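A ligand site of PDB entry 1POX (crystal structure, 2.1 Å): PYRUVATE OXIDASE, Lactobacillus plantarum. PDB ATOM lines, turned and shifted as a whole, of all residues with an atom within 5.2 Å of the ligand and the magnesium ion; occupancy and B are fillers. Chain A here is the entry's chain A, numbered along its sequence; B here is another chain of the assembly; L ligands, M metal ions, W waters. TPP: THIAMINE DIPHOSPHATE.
The backbone NH (N) of Asp 388 is in hydrogen-bond range of an oxygen (O1B) of the ligand.
An oxygen (O2A) of the ligand sits at hydrogen-bond distance from the backbone NH (N) of Gly 440 (3.3 Å).
NE2 of Gln 114 of chain B lies close to N4' of the ligand, 3.5 Å away.
N of Gly 441 sits at hydrogen-bond distance from O2A of the ligand (2.8 Å).
A nitrogen (N1') of the ligand is in hydrogen-bond range of the side-chain carboxylate of Glu 51 of chain B (2.7 Å).
O of Ala 412 is in hydrogen-bond range of N4' of the ligand.
N of Phe 471 is in hydrogen-bond range of O1B of the ligand, 2.9 Å away.
The backbone NH (N) of Gly 470 lies within hydrogen-bond range of an oxygen (O1B) of the ligand, 3.3 Å away.
The backbone carbonyl oxygen of Ala 412 is in hydrogen-bond range of the side-chain amide nitrogen of Gln 114 of chain B (3.3 Å).
OD2 of Asp 439 lies within hydrogen-bond range of N of Cys 467, at 2.8 Å.
A ring nitrogen (NE2) of His 81 of chain B is in hydrogen-bond range of the side-chain amide nitrogen (ND2) of Asn 84 (3.3 Å).
The backbone NH of Asp 439 sits at hydrogen-bond distance from the backbone carbonyl oxygen of Phe 464, at 3.2 Å.
ND2 of Asn 84 sits at hydrogen-bond distance from O of Pro 77 of chain B, at 3.2 Å.
The side-chain carboxylate (OE1) of Glu 51 of chain B is in hydrogen-bond range of a ring nitrogen (ND1) of His 81 of chain B, 2.8 Å away.
SD of Met 414 lies close to N3 of the ligand (3.7 Å).
Residues that only touch the ligand: Val 386 (3.6 Å), Gly 387 (3.9 Å), Gly 438 (3.6 Å), Met 444 (3.9 Å), Tyr 469 (3.4 Å), Ile 472 (3.5 Å), Ile 24 of chain B (3.9 Å), Pro 25 of chain B (3.4 Å), Ser 74 of chain B (3.3 Å), Pro 77 of chain B (3.5 Å), Gly 78 of chain B (3.99 Å) and His 81 of chain B (3.4 Å).
Of the 32 residues printed, 24 come within 4 Å of the ligand.
The nearest printed residue that does not touch the ligand is Thr 413 (4.2 Å).
The nearest printed residue that does not touch the magnesium ion is Gly 440 (4.1 Å).
The magnesium ion is bound by water W2, the side-chain carboxylate (OD1) of Asp 439, an oxygen (O1A) of the ligand, the backbone carbonyl oxygen (O) of Gln 468, an oxygen (O3B) of the ligand and the side-chain amide oxygen (OD1) of Asn 466.
The magnesium ion has six donor atoms within binding distance.
Water W2 lies within hydrogen-bond range of O of Phe 464 (2.7 Å), O2B of the ligand (2.9 Å), N of Asp 439 (3.3 Å) and ND2 of Asn 466 (3.4 Å).
Water W6 lies within hydrogen-bond range of an oxygen (O2A) of the ligand (2.7 Å), the backbone carbonyl oxygen of Val 386 (2.8 Å) and the backbone NH of Gly 438 (3.0 Å).
Water W4 lies within hydrogen-bond range of an oxygen (O2B) of the ligand (2.7 Å), the backbone NH of Ile 389 (2.9 Å) and the backbone NH of Asp 388 (3.3 Å).
Water W1 bridges a nitrogen (N4') of the ligand and the side-chain amide nitrogen (NE2) of Gln 114 of chain B.
Water W3 lies within hydrogen-bond range of the side-chain hydroxyl (OG) of Ser 74 of chain B (2.7 Å) and the side-chain amide oxygen (OE1) of Gln 114 of chain B (3.3 Å).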
ATOM      1  N   ASN A  84      -8.147   3.113  12.077  1.00  0.00           N
ATOM      2  CA  ASN A  84      -7.495   1.828  12.235  1.00  0.00           C
ATOM      3  C   ASN A  84      -7.296   1.118  10.919  1.00  0.00           C
ATOM      4  O   ASN A  84      -6.325   0.358  10.787  1.00  0.00           O
ATOM      5  CB  ASN A  84      -8.274   0.914  13.175  1.00  0.00           C
ATOM      6  CG  ASN A  84      -7.941   1.226  14.630  1.00  0.00           C
ATOM      7  OD1 ASN A  84      -7.960   2.380  15.077  1.00  0.00           O
ATOM      8  ND2 ASN A  84      -7.614   0.220  15.425  1.00  0.00           N
ATOM      9  N   VAL A 386      -6.797 -10.958  14.981  1.00  0.00           N
ATOM     10  CA  VAL A 386      -5.532 -10.784  15.705  1.00  0.00           C
ATOM     11  C   VAL A 386      -5.688 -11.336  17.140  1.00  0.00           C
ATOM     12  O   VAL A 386      -6.615 -10.928  17.872  1.00  0.00           O
ATOM     13  CB  VAL A 386      -5.152  -9.263  15.715  1.00  0.00           C
ATOM     14  CG1 VAL A 386      -4.009  -8.969  16.690  1.00  0.00           C
ATOM     15  CG2 VAL A 386      -4.691  -8.853  14.330  1.00  0.00           C
ATOM     16  N   GLY A 387      -4.742 -12.170  17.565  1.00  0.00           N
ATOM     17  CA  GLY A 387      -4.776 -12.768  18.893  1.00  0.00           C
ATOM     18  C   GLY A 387      -4.296 -14.195  18.767  1.00  0.00           C
ATOM     19  O   GLY A 387      -3.499 -14.481  17.845  1.00  0.00           O
ATOM     20  N   ASP A 388      -4.754 -15.142  19.603  1.00  0.00           N
ATOM     21  CA  ASP A 388      -4.326 -16.531  19.478  1.00  0.00           C
ATOM     22  C   ASP A 388      -4.610 -17.135  18.111  1.00  0.00           C
ATOM     23  O   ASP A 388      -3.854 -18.013  17.680  1.00  0.00           O
ATOM     24  CB  ASP A 388      -5.013 -17.402  20.523  1.00  0.00           C
ATOM     25  CG  ASP A 388      -4.360 -17.406  21.898  1.00  0.00           C
ATOM     26  OD1 ASP A 388      -3.237 -16.913  22.073  1.00  0.00           O
ATOM     27  OD2 ASP A 388      -4.996 -17.942  22.789  1.00  0.00           O
ATOM     28  N   ILE A 389      -5.630 -16.680  17.371  1.00  0.00           N
ATOM     29  CA  ILE A 389      -5.913 -17.194  16.026  1.00  0.00           C
ATOM     30  C   ILE A 389      -4.722 -17.046  15.092  1.00  0.00           C
ATOM     31  O   ILE A 389      -4.530 -17.936  14.267  1.00  0.00           O
ATOM     32  CB  ILE A 389      -7.231 -16.490  15.435  1.00  0.00           C
ATOM     33  CG1 ILE A 389      -7.631 -17.294  14.198  1.00  0.00           C
ATOM     34  CG2 ILE A 389      -7.061 -15.003  15.085  1.00  0.00           C
ATOM     35  CD1 ILE A 389      -7.895 -18.794  14.443  1.00  0.00           C
ATOM     36  N   ALA A 412      -1.339  -4.560  13.371  1.00  0.00           N
ATOM     37  CA  ALA A 412      -2.020  -5.598  14.134  1.00  0.00           C
ATOM     38  C   ALA A 412      -3.271  -5.145  14.880  1.00  0.00           C
ATOM     39  O   ALA A 412      -3.471  -5.385  16.070  1.00  0.00           O
ATOM     40  CB  ALA A 412      -1.028  -6.214  15.140  1.00  0.00           C
ATOM     41  N   THR A 413      -4.161  -4.509  14.126  1.00  0.00           N
ATOM     42  CA  THR A 413      -5.452  -4.080  14.630  1.00  0.00           C
ATOM     43  C   THR A 413      -6.419  -5.255  14.652  1.00  0.00           C
ATOM     44  O   THR A 413      -6.647  -5.967  13.663  1.00  0.00           O
ATOM     45  CB  THR A 413      -6.026  -2.866  13.759  1.00  0.00           C
ATOM     46  OG1 THR A 413      -7.244  -2.505  14.436  1.00  0.00           O
ATOM     47  CG2 THR A 413      -6.275  -3.145  12.251  1.00  0.00           C
ATOM     48  N   MET A 414      -7.003  -5.482  15.827  1.00  0.00           N
ATOM     49  CA  MET A 414      -8.088  -6.420  15.985  1.00  0.00           C
ATOM     50  C   MET A 414      -9.280  -5.855  15.214  1.00  0.00           C
ATOM     51  O   MET A 414      -9.399  -4.642  14.974  1.00  0.00           O
ATOM     52  CB  MET A 414      -8.492  -6.564  17.466  1.00  0.00           C
ATOM     53  CG  MET A 414      -7.454  -7.275  18.309  1.00  0.00           C
ATOM     54  SD  MET A 414      -7.779  -7.063  20.082  1.00  0.00           S
ATOM     55  CE  MET A 414      -9.388  -7.792  20.264  1.00  0.00           C
ATOM     56  N   GLY A 438     -11.097 -14.393  16.993  1.00  0.00           N
ATOM     57  CA  GLY A 438     -11.340 -14.642  18.415  1.00  0.00           C
ATOM     58  C   GLY A 438     -12.587 -13.861  18.812  1.00  0.00           C
ATOM     59  O   GLY A 438     -13.054 -12.971  18.091  1.00  0.00           O
ATOM     60  N   ASP A 439     -13.165 -14.155  19.968  1.00  0.00           N
ATOM     61  CA  ASP A 439     -14.317 -13.421  20.469  1.00  0.00           C
ATOM     62  C   ASP A 439     -14.016 -11.956  20.787  1.00  0.00           C
ATOM     63  O   ASP A 439     -14.862 -11.089  20.524  1.00  0.00           O
ATOM     64  CB  ASP A 439     -14.869 -14.131  21.701  1.00  0.00           C
ATOM     65  CG  ASP A 439     -13.915 -14.481  22.823  1.00  0.00           C
ATOM     66  OD1 ASP A 439     -12.680 -14.271  22.814  1.00  0.00           O
ATOM     67  OD2 ASP A 439     -14.414 -15.045  23.764  1.00  0.00           O
ATOM     68  N   GLY A 440     -12.829 -11.565  21.274  1.00  0.00           N
ATOM     69  CA  GLY A 440     -12.538 -10.164  21.516  1.00  0.00           C
ATOM     70  C   GLY A 440     -12.443  -9.430  20.170  1.00  0.00           C
ATOM     71  O   GLY A 440     -12.950  -8.304  20.035  1.00  0.00           O
ATOM     72  N   GLY A 441     -11.794  -9.991  19.143  1.00  0.00           N
ATOM     73  CA  GLY A 441     -11.665  -9.357  17.836  1.00  0.00           C
ATOM     74  C   GLY A 441     -12.966  -9.329  17.068  1.00  0.00           C
ATOM     75  O   GLY A 441     -13.278  -8.319  16.434  1.00  0.00           O
ATOM     76  N   ALA A 442     -13.784 -10.388  17.060  1.00  0.00           N
ATOM     77  CA  ALA A 442     -15.064 -10.383  16.356  1.00  0.00           C
ATOM     78  C   ALA A 442     -16.027  -9.412  17.046  1.00  0.00           C
ATOM     79  O   ALA A 442     -16.828  -8.773  16.325  1.00  0.00           O
ATOM     80  CB  ALA A 442     -15.735 -11.754  16.339  1.00  0.00           C
ATOM     81  N   MET A 444     -15.416  -6.439  18.212  1.00  0.00           N
ATOM     82  CA  MET A 444     -15.111  -5.064  17.846  1.00  0.00           C
ATOM     83  C   MET A 444     -15.749  -4.646  16.520  1.00  0.00           C
ATOM     84  O   MET A 444     -15.995  -3.451  16.332  1.00  0.00           O
ATOM     85  CB  MET A 444     -13.599  -4.841  17.732  1.00  0.00           C
ATOM     86  CG  MET A 444     -12.954  -4.769  19.090  1.00  0.00           C
ATOM     87  SD  MET A 444     -11.197  -4.314  19.003  1.00  0.00           S
ATOM     88  CE  MET A 444     -10.795  -4.306  20.724  1.00  0.00           C
ATOM     89  N   PHE A 464     -13.902 -18.010  17.844  1.00  0.00           N
ATOM     90  CA  PHE A 464     -13.315 -18.876  18.850  1.00  0.00           C
ATOM     91  C   PHE A 464     -13.622 -18.223  20.192  1.00  0.00           C
ATOM     92  O   PHE A 464     -12.898 -17.304  20.590  1.00  0.00           O
ATOM     93  CB  PHE A 464     -11.788 -18.960  18.589  1.00  0.00           C
ATOM     94  CG  PHE A 464     -11.430 -19.735  17.329  1.00  0.00           C
ATOM     95  CD1 PHE A 464     -11.661 -19.186  16.067  1.00  0.00           C
ATOM     96  CD2 PHE A 464     -10.922 -21.011  17.443  1.00  0.00           C
ATOM     97  CE1 PHE A 464     -11.383 -19.927  14.923  1.00  0.00           C
ATOM     98  CE2 PHE A 464     -10.643 -21.742  16.285  1.00  0.00           C
ATOM     99  CZ  PHE A 464     -10.875 -21.203  15.037  1.00  0.00           C
ATOM    100  N   ASN A 466     -13.409 -18.045  23.869  1.00  0.00           N
ATOM    101  CA  ASN A 466     -12.777 -18.523  25.088  1.00  0.00           C
ATOM    102  C   ASN A 466     -13.145 -17.622  26.280  1.00  0.00           C
ATOM    103  O   ASN A 466     -12.671 -17.872  27.397  1.00  0.00           O
ATOM    104  CB  ASN A 466     -11.233 -18.609  24.969  1.00  0.00           C
ATOM    105  CG  ASN A 466     -10.490 -17.406  24.403  1.00  0.00           C
ATOM    106  OD1 ASN A 466     -11.013 -16.287  24.225  1.00  0.00           O
ATOM    107  ND2 ASN A 466      -9.227 -17.586  24.054  1.00  0.00           N
ATOM    108  N   CYS A 467     -13.974 -16.577  26.118  1.00  0.00           N
ATOM    109  CA  CYS A 467     -14.318 -15.588  27.155  1.00  0.00           C
ATOM    110  C   CYS A 467     -13.073 -14.924  27.779  1.00  0.00           C
ATOM    111  O   CYS A 467     -12.978 -14.544  28.952  1.00  0.00           O
ATOM    112  CB  CYS A 467     -15.198 -16.236  28.255  1.00  0.00           C
ATOM    113  SG  CYS A 467     -16.869 -16.648  27.654  1.00  0.00           S
ATOM    114  N   GLN A 468     -12.112 -14.691  26.889  1.00  0.00           N
ATOM    115  CA  GLN A 468     -10.824 -14.109  27.259  1.00  0.00           C
ATOM    116  C   GLN A 468     -10.210 -13.377  26.093  1.00  0.00           C
ATOM    117  O   GLN A 468     -10.504 -13.688  24.900  1.00  0.00           O
ATOM    118  CB  GLN A 468      -9.771 -15.126  27.614  1.00  0.00           C
ATOM    119  CG  GLN A 468     -10.060 -16.093  28.695  1.00  0.00           C
ATOM    120  CD  GLN A 468      -8.998 -17.163  28.770  1.00  0.00           C
ATOM    121  OE1 GLN A 468      -8.986 -17.913  29.730  1.00  0.00           O
ATOM    122  NE2 GLN A 468      -8.013 -17.366  27.919  1.00  0.00           N
ATOM    123  N   TYR A 469      -9.330 -12.459  26.491  1.00  0.00           N
ATOM    124  CA  TYR A 469      -8.348 -11.921  25.572  1.00  0.00           C
ATOM    125  C   TYR A 469      -7.169 -12.901  25.824  1.00  0.00           C
ATOM    126  O   TYR A 469      -6.232 -12.618  26.571  1.00  0.00           O
ATOM    127  CB  TYR A 469      -7.910 -10.472  25.936  1.00  0.00           C
ATOM    128  CG  TYR A 469      -8.961  -9.395  25.667  1.00  0.00           C
ATOM    129  CD1 TYR A 469      -9.548  -9.288  24.415  1.00  0.00           C
ATOM    130  CD2 TYR A 469      -9.364  -8.551  26.693  1.00  0.00           C
ATOM    131  CE1 TYR A 469     -10.540  -8.356  24.162  1.00  0.00           C
ATOM    132  CE2 TYR A 469     -10.350  -7.595  26.444  1.00  0.00           C
ATOM    133  CZ  TYR A 469     -10.935  -7.506  25.188  1.00  0.00           C
ATOM    134  OH  TYR A 469     -11.916  -6.553  24.951  1.00  0.00           O
ATOM    135  N   GLY A 470      -7.199 -14.096  25.214  1.00  0.00           N
ATOM    136  CA  GLY A 470      -6.255 -15.154  25.536  1.00  0.00           C
ATOM    137  C   GLY A 470      -4.802 -14.743  25.272  1.00  0.00           C
ATOM    138  O   GLY A 470      -3.923 -15.002  26.117  1.00  0.00           O
ATOM    139  N   PHE A 471      -4.494 -14.098  24.126  1.00  0.00           N
ATOM    140  CA  PHE A 471      -3.130 -13.664  23.821  1.00  0.00           C
ATOM    141  C   PHE A 471      -2.594 -12.698  24.902  1.00  0.00           C
ATOM    142  O   PHE A 471      -1.412 -12.756  25.216  1.00  0.00           O
ATOM    143  CB  PHE A 471      -3.126 -12.977  22.425  1.00  0.00           C
ATOM    144  CG  PHE A 471      -1.837 -13.019  21.549  1.00  0.00           C
ATOM    145  CD1 PHE A 471      -1.407 -14.204  20.957  1.00  0.00           C
ATOM    146  CD2 PHE A 471      -1.104 -11.869  21.300  1.00  0.00           C
ATOM    147  CE1 PHE A 471      -0.289 -14.219  20.134  1.00  0.00           C
ATOM    148  CE2 PHE A 471       0.020 -11.890  20.480  1.00  0.00           C
ATOM    149  CZ  PHE A 471       0.435 -13.059  19.891  1.00  0.00           C
ATOM    150  N   ILE A 472      -3.412 -11.842  25.546  1.00  0.00           N
ATOM    151  CA  ILE A 472      -2.911 -10.911  26.571  1.00  0.00           C
ATOM    152  C   ILE A 472      -2.821 -11.565  27.958  1.00  0.00           C
ATOM    153  O   ILE A 472      -1.898 -11.285  28.757  1.00  0.00           O
ATOM    154  CB  ILE A 472      -3.833  -9.639  26.626  1.00  0.00           C
ATOM    155  CG1 ILE A 472      -3.969  -9.027  25.226  1.00  0.00           C
ATOM    156  CG2 ILE A 472      -3.247  -8.581  27.565  1.00  0.00           C
ATOM    157  CD1 ILE A 472      -2.685  -8.745  24.418  1.00  0.00           C
ATOM    158  N   PHE A 489     -13.643 -12.199  30.686  1.00  0.00           N
ATOM    159  CA  PHE A 489     -14.819 -11.360  30.612  1.00  0.00           C
ATOM    160  C   PHE A 489     -16.080 -12.167  30.325  1.00  0.00           C
ATOM    161  O   PHE A 489     -16.001 -13.399  30.149  1.00  0.00           O
ATOM    162  CB  PHE A 489     -14.600 -10.298  29.499  1.00  0.00           C
ATOM    163  CG  PHE A 489     -14.097 -10.768  28.130  1.00  0.00           C
ATOM    164  CD1 PHE A 489     -14.850 -11.611  27.328  1.00  0.00           C
ATOM    165  CD2 PHE A 489     -12.872 -10.308  27.679  1.00  0.00           C
ATOM    166  CE1 PHE A 489     -14.358 -11.984  26.084  1.00  0.00           C
ATOM    167  CE2 PHE A 489     -12.396 -10.692  26.448  1.00  0.00           C
ATOM    168  CZ  PHE A 489     -13.136 -11.518  25.652  1.00  0.00           C
ATOM    169  N   ILE B  24      -8.729  -1.335  27.460  1.00  0.00           N
ATOM    170  CA  ILE B  24      -8.539  -2.719  27.022  1.00  0.00           C
ATOM    171  C   ILE B  24      -7.040  -2.957  27.133  1.00  0.00           C
ATOM    172  O   ILE B  24      -6.285  -2.090  26.676  1.00  0.00           O
ATOM    173  CB  ILE B  24      -9.030  -2.890  25.539  1.00  0.00           C
ATOM    174  CG1 ILE B  24     -10.531  -2.732  25.521  1.00  0.00           C
ATOM    175  CG2 ILE B  24      -8.573  -4.231  24.952  1.00  0.00           C
ATOM    176  CD1 ILE B  24     -11.173  -2.961  24.122  1.00  0.00           C
ATOM    177  N   PRO B  25      -6.532  -4.026  27.751  1.00  0.00           N
ATOM    178  CA  PRO B  25      -5.103  -4.256  27.966  1.00  0.00           C
ATOM    179  C   PRO B  25      -4.385  -4.708  26.696  1.00  0.00           C
ATOM    180  O   PRO B  25      -4.971  -5.113  25.698  1.00  0.00           O
ATOM    181  CB  PRO B  25      -5.071  -5.289  29.061  1.00  0.00           C
ATOM    182  CG  PRO B  25      -6.305  -6.119  28.733  1.00  0.00           C
ATOM    183  CD  PRO B  25      -7.343  -5.052  28.416  1.00  0.00           C
ATOM    184  N   GLY B  26      -3.083  -4.680  26.771  1.00  0.00           N
ATOM    185  CA  GLY B  26      -2.238  -5.134  25.690  1.00  0.00           C
ATOM    186  C   GLY B  26      -0.873  -5.230  26.309  1.00  0.00           C
ATOM    187  O   GLY B  26      -0.615  -4.633  27.376  1.00  0.00           O
ATOM    188  N   GLU B  51     -12.248   0.303  22.311  1.00  0.00           N
ATOM    189  CA  GLU B  51     -11.673   1.440  23.028  1.00  0.00           C
ATOM    190  C   GLU B  51     -12.317   2.789  22.731  1.00  0.00           C
ATOM    191  O   GLU B  51     -12.185   3.697  23.574  1.00  0.00           O
ATOM    192  CB  GLU B  51     -10.164   1.610  22.782  1.00  0.00           C
ATOM    193  CG  GLU B  51      -9.270   0.450  23.133  1.00  0.00           C
ATOM    194  CD  GLU B  51      -9.074  -0.600  22.043  1.00  0.00           C
ATOM    195  OE1 GLU B  51      -9.826  -0.657  21.071  1.00  0.00           O
ATOM    196  OE2 GLU B  51      -8.186  -1.420  22.188  1.00  0.00           O
ATOM    197  N   SER B  74      -3.834   0.474  24.244  1.00  0.00           N
ATOM    198  CA  SER B  74      -2.516  -0.084  24.014  1.00  0.00           C
ATOM    199  C   SER B  74      -1.902   0.558  22.761  1.00  0.00           C
ATOM    200  O   SER B  74      -2.576   1.294  22.023  1.00  0.00           O
ATOM    201  CB  SER B  74      -2.637  -1.609  23.871  1.00  0.00           C
ATOM    202  OG  SER B  74      -3.628  -1.957  22.893  1.00  0.00           O
ATOM    203  N   PRO B  77      -3.087   0.349  17.367  1.00  0.00           N
ATOM    204  CA  PRO B  77      -4.521   0.309  17.214  1.00  0.00           C
ATOM    205  C   PRO B  77      -5.373   0.533  18.471  1.00  0.00           C
ATOM    206  O   PRO B  77      -6.545   0.895  18.340  1.00  0.00           O
ATOM    207  CB  PRO B  77      -4.694  -1.032  16.528  1.00  0.00           C
ATOM    208  CG  PRO B  77      -3.634  -1.902  17.131  1.00  0.00           C
ATOM    209  CD  PRO B  77      -2.475  -0.947  17.063  1.00  0.00           C
ATOM    210  N   GLY B  78      -4.877   0.310  19.687  1.00  0.00           N
ATOM    211  CA  GLY B  78      -5.632   0.584  20.897  1.00  0.00           C
ATOM    212  C   GLY B  78      -5.864   2.077  21.024  1.00  0.00           C
ATOM    213  O   GLY B  78      -6.985   2.561  21.179  1.00  0.00           O
ATOM    214  N   HIS B  81      -8.116   3.835  18.221  1.00  0.00           N
ATOM    215  CA  HIS B  81      -9.512   3.560  18.444  1.00  0.00           C
ATOM    216  C   HIS B  81     -10.142   4.599  19.360  1.00  0.00           C
ATOM    217  O   HIS B  81     -11.364   4.759  19.337  1.00  0.00           O
ATOM    218  CB  HIS B  81      -9.781   2.180  19.096  1.00  0.00           C
ATOM    219  CG  HIS B  81     -10.186   1.051  18.154  1.00  0.00           C
ATOM    220  ND1 HIS B  81     -10.291  -0.253  18.384  1.00  0.00           N
ATOM    221  CD2 HIS B  81     -10.509   1.220  16.830  1.00  0.00           C
ATOM    222  CE1 HIS B  81     -10.651  -0.866  17.288  1.00  0.00           C
ATOM    223  NE2 HIS B  81     -10.771   0.030  16.357  1.00  0.00           N
ATOM    224  N   GLN B 114       4.446  -3.517  16.225  1.00  0.00           N
ATOM    225  CA  GLN B 114       3.461  -2.525  16.637  1.00  0.00           C
ATOM    226  C   GLN B 114       4.094  -1.308  17.323  1.00  0.00           C
ATOM    227  O   GLN B 114       3.546  -0.747  18.290  1.00  0.00           O
ATOM    228  CB  GLN B 114       2.458  -3.260  17.547  1.00  0.00           C
ATOM    229  CG  GLN B 114       1.081  -2.674  17.620  1.00  0.00           C
ATOM    230  CD  GLN B 114       0.164  -3.620  18.360  1.00  0.00           C
ATOM    231  OE1 GLN B 114       0.483  -4.142  19.422  1.00  0.00           O
ATOM    232  NE2 GLN B 114      -0.988  -3.961  17.807  1.00  0.00           N
HETATM  233  N1' TPP L   1      -6.824  -3.223  20.777  1.00  0.00           N
HETATM  234  C2' TPP L   1      -6.768  -3.285  19.449  1.00  0.00           C
HETATM  235  CM2 TPP L   1      -7.783  -2.543  18.587  1.00  0.00           C
HETATM  236  N3' TPP L   1      -5.831  -4.010  18.840  1.00  0.00           N
HETATM  237  C4' TPP L   1      -4.898  -4.701  19.544  1.00  0.00           C
HETATM  238  N4' TPP L   1      -3.967  -5.392  18.858  1.00  0.00           N
HETATM  239  C5' TPP L   1      -5.005  -4.714  20.956  1.00  0.00           C
HETATM  240  C6' TPP L   1      -5.979  -3.911  21.554  1.00  0.00           C
HETATM  241  C7' TPP L   1      -4.097  -5.570  21.854  1.00  0.00           C
HETATM  242  N3  TPP L   1      -4.419  -7.008  21.695  1.00  0.00           N
HETATM  243  C2  TPP L   1      -3.674  -7.746  20.914  1.00  0.00           C
HETATM  244  S1  TPP L   1      -4.193  -9.429  20.910  1.00  0.00           S
HETATM  245  C5  TPP L   1      -5.515  -8.964  21.985  1.00  0.00           C
HETATM  246  C4  TPP L   1      -5.429  -7.657  22.296  1.00  0.00           C
HETATM  247  CM4 TPP L   1      -6.399  -7.001  23.245  1.00  0.00           C
HETATM  248  C6  TPP L   1      -6.544  -9.931  22.492  1.00  0.00           C
HETATM  249  C7  TPP L   1      -7.150 -10.786  21.383  1.00  0.00           C
HETATM  250  O7  TPP L   1      -8.443 -11.355  21.949  1.00  0.00           O
HETATM  251  PA  TPP L   1      -9.334 -12.363  21.207  1.00  0.00           P
HETATM  252  O1A TPP L   1     -10.390 -12.810  22.126  1.00  0.00           O
HETATM  253  O2A TPP L   1      -9.764 -11.798  19.943  1.00  0.00           O
HETATM  254  O3A TPP L   1      -8.380 -13.611  20.945  1.00  0.00           O
HETATM  255  PB  TPP L   1      -7.803 -14.845  21.801  1.00  0.00           P
HETATM  256  O1B TPP L   1      -6.413 -14.536  22.057  1.00  0.00           O
HETATM  257  O2B TPP L   1      -8.003 -15.936  20.863  1.00  0.00           O
HETATM  258  O3B TPP L   1      -8.693 -14.942  22.995  1.00  0.00           O
HETATM  259 MG    MG M   1     -10.707 -14.556  23.081  1.00  0.00          MG
HETATM  260  O   HOH W   1      -1.354  -6.368  19.223  1.00  0.00           O
HETATM  261  O   HOH W   2     -10.782 -15.856  21.550  1.00  0.00           O
HETATM  262  O   HOH W   3      -2.325  -2.829  20.676  1.00  0.00           O
HETATM  263  O   HOH W   4      -7.821 -14.966  18.313  1.00  0.00           O
HETATM  264  O   HOH W   5      -1.340  -9.256  19.236  1.00  0.00           O
HETATM  265  O   HOH W   6      -9.007 -12.342  17.385  1.00  0.00           O
HETATM  266  O   HOH W   7      -8.405 -18.698  20.411  1.00  0.00           O
